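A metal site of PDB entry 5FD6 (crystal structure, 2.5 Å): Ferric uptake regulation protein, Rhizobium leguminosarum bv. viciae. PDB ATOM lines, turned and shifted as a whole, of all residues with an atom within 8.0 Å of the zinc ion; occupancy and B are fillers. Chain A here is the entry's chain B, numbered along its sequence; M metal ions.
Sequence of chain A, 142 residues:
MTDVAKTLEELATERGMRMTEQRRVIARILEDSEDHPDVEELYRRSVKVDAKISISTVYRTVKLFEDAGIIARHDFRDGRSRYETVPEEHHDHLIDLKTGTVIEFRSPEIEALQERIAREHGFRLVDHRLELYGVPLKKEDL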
ATOM      1  N   GLU A  34      -8.094  -1.143  17.281  1.00  0.00           N
ATOM      2  CA  GLU A  34      -7.120  -1.676  18.239  1.00  0.00           C
ATOM      3  C   GLU A  34      -7.582  -2.997  18.832  1.00  0.00           C
ATOM      4  O   GLU A  34      -6.802  -3.660  19.520  1.00  0.00           O
ATOM      5  CB  GLU A  34      -6.837  -0.674  19.364  1.00  0.00           C
ATOM      6  CG  GLU A  34      -5.457  -0.810  20.020  1.00  0.00           C
ATOM      7  CD  GLU A  34      -4.287  -0.351  19.147  1.00  0.00           C
ATOM      8  OE1 GLU A  34      -4.470   0.558  18.305  1.00  0.00           O
ATOM      9  OE2 GLU A  34      -3.177  -0.919  19.303  1.00  0.00           O
ATOM     10  N   ASP A  35      -8.833  -3.387  18.598  1.00  0.00           N
ATOM     11  CA  ASP A  35      -9.226  -4.777  18.842  1.00  0.00           C
ATOM     12  C   ASP A  35      -8.504  -5.657  17.816  1.00  0.00           C
ATOM     13  O   ASP A  35      -7.581  -5.189  17.126  1.00  0.00           O
ATOM     14  CB  ASP A  35     -10.763  -4.968  18.926  1.00  0.00           C
ATOM     15  CG  ASP A  35     -11.497  -4.739  17.616  1.00  0.00           C
ATOM     16  OD1 ASP A  35     -10.895  -4.354  16.587  1.00  0.00           O
ATOM     17  OD2 ASP A  35     -12.723  -4.953  17.634  1.00  0.00           O
ATOM     18  N   HIS A  36      -8.855  -6.920  17.714  1.00  0.00           N
ATOM     19  CA  HIS A  36      -8.078  -7.816  16.886  1.00  0.00           C
ATOM     20  C   HIS A  36      -9.026  -8.392  15.875  1.00  0.00           C
ATOM     21  O   HIS A  36      -9.340  -9.554  15.938  1.00  0.00           O
ATOM     22  CB  HIS A  36      -7.415  -8.881  17.766  1.00  0.00           C
ATOM     23  CG  HIS A  36      -6.102  -8.439  18.298  1.00  0.00           C
ATOM     24  ND1 HIS A  36      -5.957  -7.811  19.517  1.00  0.00           N
ATOM     25  CD2 HIS A  36      -4.867  -8.465  17.744  1.00  0.00           C
ATOM     26  CE1 HIS A  36      -4.689  -7.506  19.696  1.00  0.00           C
ATOM     27  NE2 HIS A  36      -4.008  -7.892  18.643  1.00  0.00           N
ATOM     28  N   ALA A  72      -0.449  -7.763  10.282  1.00  0.00           N
ATOM     29  CA  ALA A  72      -0.171  -9.111  10.756  1.00  0.00           C
ATOM     30  C   ALA A  72      -1.414  -9.988  10.883  1.00  0.00           C
ATOM     31  O   ALA A  72      -2.427  -9.549  11.412  1.00  0.00           O
ATOM     32  CB  ALA A  72       0.533  -9.044  12.112  1.00  0.00           C
ATOM     33  N   HIS A  74      -2.825 -13.347  12.857  1.00  0.00           N
ATOM     34  CA  HIS A  74      -2.639 -14.323  13.925  1.00  0.00           C
ATOM     35  C   HIS A  74      -3.708 -15.395  13.840  1.00  0.00           C
ATOM     36  O   HIS A  74      -4.900 -15.111  13.971  1.00  0.00           O
ATOM     37  CB  HIS A  74      -2.631 -13.658  15.306  1.00  0.00           C
ATOM     38  CG  HIS A  74      -1.444 -12.775  15.537  1.00  0.00           C
ATOM     39  ND1 HIS A  74      -0.168 -13.279  15.666  1.00  0.00           N
ATOM     40  CD2 HIS A  74      -1.331 -11.431  15.614  1.00  0.00           C
ATOM     41  CE1 HIS A  74       0.688 -12.273  15.824  1.00  0.00           C
ATOM     42  NE2 HIS A  74       0.003 -11.148  15.804  1.00  0.00           N
ATOM     43  N   PHE A  76      -5.163 -17.978  15.770  1.00  0.00           N
ATOM     44  CA  PHE A  76      -5.268 -18.492  17.118  1.00  0.00           C
ATOM     45  C   PHE A  76      -5.997 -19.825  17.166  1.00  0.00           C
ATOM     46  O   PHE A  76      -6.793 -20.135  16.296  1.00  0.00           O
ATOM     47  CB  PHE A  76      -5.948 -17.452  18.007  1.00  0.00           C
ATOM     48  CG  PHE A  76      -5.156 -16.179  18.155  1.00  0.00           C
ATOM     49  CD1 PHE A  76      -3.825 -16.212  18.557  1.00  0.00           C
ATOM     50  CD2 PHE A  76      -5.743 -14.935  17.923  1.00  0.00           C
ATOM     51  CE1 PHE A  76      -3.093 -15.049  18.714  1.00  0.00           C
ATOM     52  CE2 PHE A  76      -5.015 -13.760  18.085  1.00  0.00           C
ATOM     53  CZ  PHE A  76      -3.685 -13.820  18.473  1.00  0.00           C
ATOM     54  N   ARG A  82      -7.023 -13.465  13.203  1.00  0.00           N
ATOM     55  CA  ARG A  82      -7.260 -12.082  13.648  1.00  0.00           C
ATOM     56  C   ARG A  82      -6.185 -11.158  13.096  1.00  0.00           C
ATOM     57  O   ARG A  82      -5.128 -11.636  12.731  1.00  0.00           O
ATOM     58  CB  ARG A  82      -7.445 -12.069  15.167  1.00  0.00           C
ATOM     59  CG  ARG A  82      -8.838 -12.578  15.487  1.00  0.00           C
ATOM     60  CD  ARG A  82      -9.080 -13.115  16.863  1.00  0.00           C
ATOM     61  NE  ARG A  82     -10.512 -13.033  17.131  1.00  0.00           N
ATOM     62  CZ  ARG A  82     -11.172 -11.917  17.472  1.00  0.00           C
ATOM     63  NH1 ARG A  82     -10.534 -10.756  17.636  1.00  0.00           N
ATOM     64  NH2 ARG A  82     -12.493 -11.943  17.665  1.00  0.00           N
ATOM     65  N   TYR A  83      -6.505  -9.875  12.931  1.00  0.00           N
ATOM     66  CA  TYR A  83      -5.612  -8.937  12.181  1.00  0.00           C
ATOM     67  C   TYR A  83      -5.343  -7.664  12.967  1.00  0.00           C
ATOM     68  O   TYR A  83      -6.185  -7.214  13.728  1.00  0.00           O
ATOM     69  CB  TYR A  83      -6.156  -8.571  10.781  1.00  0.00           C
ATOM     70  CG  TYR A  83      -6.294  -9.739   9.809  1.00  0.00           C
ATOM     71  CD1 TYR A  83      -5.335  -9.978   8.798  1.00  0.00           C
ATOM     72  CD2 TYR A  83      -7.387 -10.588   9.865  1.00  0.00           C
ATOM     73  CE1 TYR A  83      -5.464 -11.050   7.915  1.00  0.00           C
ATOM     74  CE2 TYR A  83      -7.530 -11.658   8.985  1.00  0.00           C
ATOM     75  CZ  TYR A  83      -6.590 -11.883   8.007  1.00  0.00           C
ATOM     76  OH  TYR A  83      -6.779 -12.963   7.152  1.00  0.00           O
ATOM     77  N   GLU A  84      -4.147  -7.108  12.770  1.00  0.00           N
ATOM     78  CA  GLU A  84      -3.735  -5.829  13.393  1.00  0.00           C
ATOM     79  C   GLU A  84      -2.676  -5.191  12.493  1.00  0.00           C
ATOM     80  O   GLU A  84      -2.128  -5.858  11.610  1.00  0.00           O
ATOM     81  CB  GLU A  84      -3.203  -6.035  14.819  1.00  0.00           C
ATOM     82  CG  GLU A  84      -2.101  -7.090  14.897  1.00  0.00           C
ATOM     83  CD  GLU A  84      -1.606  -7.328  16.315  1.00  0.00           C
ATOM     84  OE1 GLU A  84      -1.391  -8.505  16.694  1.00  0.00           O
ATOM     85  OE2 GLU A  84      -1.442  -6.338  17.068  1.00  0.00           O
ATOM     86  N   THR A  85      -2.378  -3.917  12.732  1.00  0.00           N
ATOM     87  CA  THR A  85      -1.647  -3.066  11.774  1.00  0.00           C
ATOM     88  C   THR A  85      -0.098  -3.114  11.855  1.00  0.00           C
ATOM     89  O   THR A  85       0.566  -2.140  11.484  1.00  0.00           O
ATOM     90  CB  THR A  85      -2.110  -1.606  11.895  1.00  0.00           C
ATOM     91  OG1 THR A  85      -1.957  -1.152  13.251  1.00  0.00           O
ATOM     92  CG2 THR A  85      -3.554  -1.482  11.514  1.00  0.00           C
ATOM     93  N   VAL A  86       0.453  -4.250  12.257  1.00  0.00           N
ATOM     94  CA  VAL A  86       1.829  -4.329  12.777  1.00  0.00           C
ATOM     95  C   VAL A  86       1.964  -3.277  13.868  1.00  0.00           C
ATOM     96  O   VAL A  86       2.767  -2.339  13.716  1.00  0.00           O
ATOM     97  CB  VAL A  86       2.919  -4.134  11.693  1.00  0.00           C
ATOM     98  CG1 VAL A  86       4.317  -4.387  12.235  1.00  0.00           C
ATOM     99  CG2 VAL A  86       2.708  -5.071  10.523  1.00  0.00           C
ATOM    100  N   PRO A  87       1.156  -3.382  14.958  1.00  0.00           N
ATOM    101  CA  PRO A  87       1.387  -2.456  16.071  1.00  0.00           C
ATOM    102  C   PRO A  87       2.844  -2.444  16.504  1.00  0.00           C
ATOM    103  O   PRO A  87       3.477  -3.496  16.625  1.00  0.00           O
ATOM    104  CB  PRO A  87       0.453  -2.990  17.162  1.00  0.00           C
ATOM    105  CG  PRO A  87      -0.704  -3.472  16.370  1.00  0.00           C
ATOM    106  CD  PRO A  87      -0.050  -4.192  15.215  1.00  0.00           C
ATOM    107  N   GLU A  89       4.559  -1.774  19.132  1.00  0.00           N
ATOM    108  CA  GLU A  89       4.932  -2.496  20.342  1.00  0.00           C
ATOM    109  C   GLU A  89       4.883  -3.994  20.119  1.00  0.00           C
ATOM    110  O   GLU A  89       3.983  -4.501  19.451  1.00  0.00           O
ATOM    111  CB  GLU A  89       4.022  -2.152  21.534  1.00  0.00           C
ATOM    112  CG  GLU A  89       4.525  -1.015  22.427  1.00  0.00           C
ATOM    113  CD  GLU A  89       5.697  -1.429  23.307  1.00  0.00           C
ATOM    114  OE1 GLU A  89       5.445  -2.072  24.363  1.00  0.00           O
ATOM    115  OE2 GLU A  89       6.854  -1.116  22.964  1.00  0.00           O
ATOM    116  N   HIS A  90       5.867  -4.696  20.672  1.00  0.00           N
ATOM    117  CA  HIS A  90       5.723  -6.111  20.949  1.00  0.00           C
ATOM    118  C   HIS A  90       4.670  -6.248  22.056  1.00  0.00           C
ATOM    119  O   HIS A  90       4.623  -5.453  22.997  1.00  0.00           O
ATOM    120  CB  HIS A  90       7.051  -6.730  21.414  1.00  0.00           C
ATOM    121  CG  HIS A  90       6.877  -8.076  22.050  1.00  0.00           C
ATOM    122  ND1 HIS A  90       7.029  -9.258  21.352  1.00  0.00           N
ATOM    123  CD2 HIS A  90       6.493  -8.425  23.304  1.00  0.00           C
ATOM    124  CE1 HIS A  90       6.779 -10.272  22.154  1.00  0.00           C
ATOM    125  NE2 HIS A  90       6.449  -9.796  23.340  1.00  0.00           N
ATOM    126  N   HIS A  91       3.805  -7.247  21.914  1.00  0.00           N
ATOM    127  CA  HIS A  91       2.885  -7.686  22.975  1.00  0.00           C
ATOM    128  C   HIS A  91       2.486  -9.142  22.714  1.00  0.00           C
ATOM    129  O   HIS A  91       2.576  -9.628  21.575  1.00  0.00           O
ATOM    130  CB  HIS A  91       1.655  -6.784  23.068  1.00  0.00           C
ATOM    131  CG  HIS A  91       0.844  -6.702  21.810  1.00  0.00           C
ATOM    132  ND1 HIS A  91       1.296  -6.120  20.650  1.00  0.00           N
ATOM    133  CD2 HIS A  91      -0.415  -7.136  21.540  1.00  0.00           C
ATOM    134  CE1 HIS A  91       0.366  -6.199  19.718  1.00  0.00           C
ATOM    135  NE2 HIS A  91      -0.684  -6.808  20.231  1.00  0.00           N
ATOM    136  N   ASP A  92       2.084  -9.841  23.766  1.00  0.00           N
ATOM    137  CA  ASP A  92       1.559 -11.214  23.656  1.00  0.00           C
ATOM    138  C   ASP A  92       0.050 -11.200  23.808  1.00  0.00           C
ATOM    139  O   ASP A  92      -0.535 -10.120  23.888  1.00  0.00           O
ATOM    140  CB  ASP A  92       2.221 -12.115  24.690  1.00  0.00           C
ATOM    141  CG  ASP A  92       3.707 -12.042  24.624  1.00  0.00           C
ATOM    142  OD1 ASP A  92       4.250 -12.105  23.495  1.00  0.00           O
ATOM    143  OD2 ASP A  92       4.342 -11.896  25.687  1.00  0.00           O
ATOM    144  N   HIS A  93      -0.573 -12.379  23.831  1.00  0.00           N
ATOM    145  CA  HIS A  93      -2.021 -12.504  23.646  1.00  0.00           C
ATOM    146  C   HIS A  93      -2.685 -13.489  24.598  1.00  0.00           C
ATOM    147  O   HIS A  93      -2.134 -14.556  24.897  1.00  0.00           O
ATOM    148  CB  HIS A  93      -2.317 -12.963  22.220  1.00  0.00           C
ATOM    149  CG  HIS A  93      -1.969 -11.942  21.166  1.00  0.00           C
ATOM    150  ND1 HIS A  93      -0.789 -11.976  20.461  1.00  0.00           N
ATOM    151  CD2 HIS A  93      -2.654 -10.887  20.694  1.00  0.00           C
ATOM    152  CE1 HIS A  93      -0.761 -10.986  19.587  1.00  0.00           C
ATOM    153  NE2 HIS A  93      -1.881 -10.300  19.721  1.00  0.00           N
ATOM    154  N   VAL A 102      -9.808 -10.702  22.460  1.00  0.00           N
ATOM    155  CA  VAL A 102      -8.346 -10.822  22.532  1.00  0.00           C
ATOM    156  C   VAL A 102      -7.858  -9.746  23.490  1.00  0.00           C
ATOM    157  O   VAL A 102      -8.050  -8.570  23.259  1.00  0.00           O
ATOM    158  CB  VAL A 102      -7.711 -10.633  21.147  1.00  0.00           C
ATOM    159  CG1 VAL A 102      -6.193 -10.672  21.219  1.00  0.00           C
ATOM    160  CG2 VAL A 102      -8.200 -11.710  20.189  1.00  0.00           C
ATOM    161  N   ILE A 103      -7.237 -10.163  24.587  1.00  0.00           N
ATOM    162  CA  ILE A 103      -6.687  -9.269  25.581  1.00  0.00           C
ATOM    163  C   ILE A 103      -5.180  -9.294  25.395  1.00  0.00           C
ATOM    164  O   ILE A 103      -4.552 -10.343  25.524  1.00  0.00           O
ATOM    165  CB  ILE A 103      -7.065  -9.709  26.997  1.00  0.00           C
ATOM    166  CG1 ILE A 103      -8.593  -9.873  27.099  1.00  0.00           C
ATOM    167  CG2 ILE A 103      -6.544  -8.708  28.017  1.00  0.00           C
ATOM    168  CD1 ILE A 103      -9.134 -10.155  28.479  1.00  0.00           C
ATOM    169  N   GLU A 104      -4.611  -8.140  25.092  1.00  0.00           N
ATOM    170  CA  GLU A 104      -3.160  -8.019  24.889  1.00  0.00           C
ATOM    171  C   GLU A 104      -2.430  -7.723  26.205  1.00  0.00           C
ATOM    172  O   GLU A 104      -2.992  -7.125  27.131  1.00  0.00           O
ATOM    173  CB  GLU A 104      -2.792  -7.018  23.781  1.00  0.00           C
ATOM    174  CG  GLU A 104      -3.554  -5.703  23.687  1.00  0.00           C
ATOM    175  CD  GLU A 104      -3.169  -4.910  22.451  1.00  0.00           C
ATOM    176  OE1 GLU A 104      -1.990  -4.538  22.331  1.00  0.00           O
ATOM    177  OE2 GLU A 104      -4.039  -4.643  21.600  1.00  0.00           O
ATOM    178  N   PHE A 105      -1.196  -8.221  26.283  1.00  0.00           N
ATOM    179  CA  PHE A 105      -0.378  -8.044  27.465  1.00  0.00           C
ATOM    180  C   PHE A 105       1.106  -8.119  27.139  1.00  0.00           C
ATOM    181  O   PHE A 105       1.508  -8.567  26.070  1.00  0.00           O
ATOM    182  CB  PHE A 105      -0.787  -9.029  28.579  1.00  0.00           C
ATOM    183  CG  PHE A 105      -0.279 -10.438  28.402  1.00  0.00           C
ATOM    184  CD1 PHE A 105       0.764 -10.928  29.199  1.00  0.00           C
ATOM    185  CD2 PHE A 105      -0.839 -11.291  27.460  1.00  0.00           C
ATOM    186  CE1 PHE A 105       1.230 -12.227  29.052  1.00  0.00           C
ATOM    187  CE2 PHE A 105      -0.368 -12.594  27.304  1.00  0.00           C
ATOM    188  CZ  PHE A 105       0.676 -13.065  28.094  1.00  0.00           C
HETATM  189 ZN    ZN M   1      -1.806  -8.187  18.803  1.00  0.00          ZN
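The zinc ion is bound by OE1 of Glu 84, NE2 of His 36, NE2 of His 91, NE2 of His 93 and OE2 of Glu 84.
The zinc ion has five donor atoms within binding distance.
Within 4 Å of the zinc ion: His 36, Glu 84, His 91 and His 93.
The nearest printed residue that does not touch the zinc ion is His 74 (4.6 Å).
The side-chain carboxylate (OE1) of Glu 84 sits close to a ring nitrogen (NE2) of His 74 (3.1 Å).
O of Glu 84 lies within hydrogen-bond range of N of Ala 72, at 2.9 Å.
The side-chain carboxylate (OE1) of Glu 104 lies close to a ring nitrogen (NE2) of His 91, at 3.4 Å.
The backbone carbonyl oxygen (O) of Glu 89 is in hydrogen-bond range of a ring nitrogen (ND1) of His 91, 3.4 Å away.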
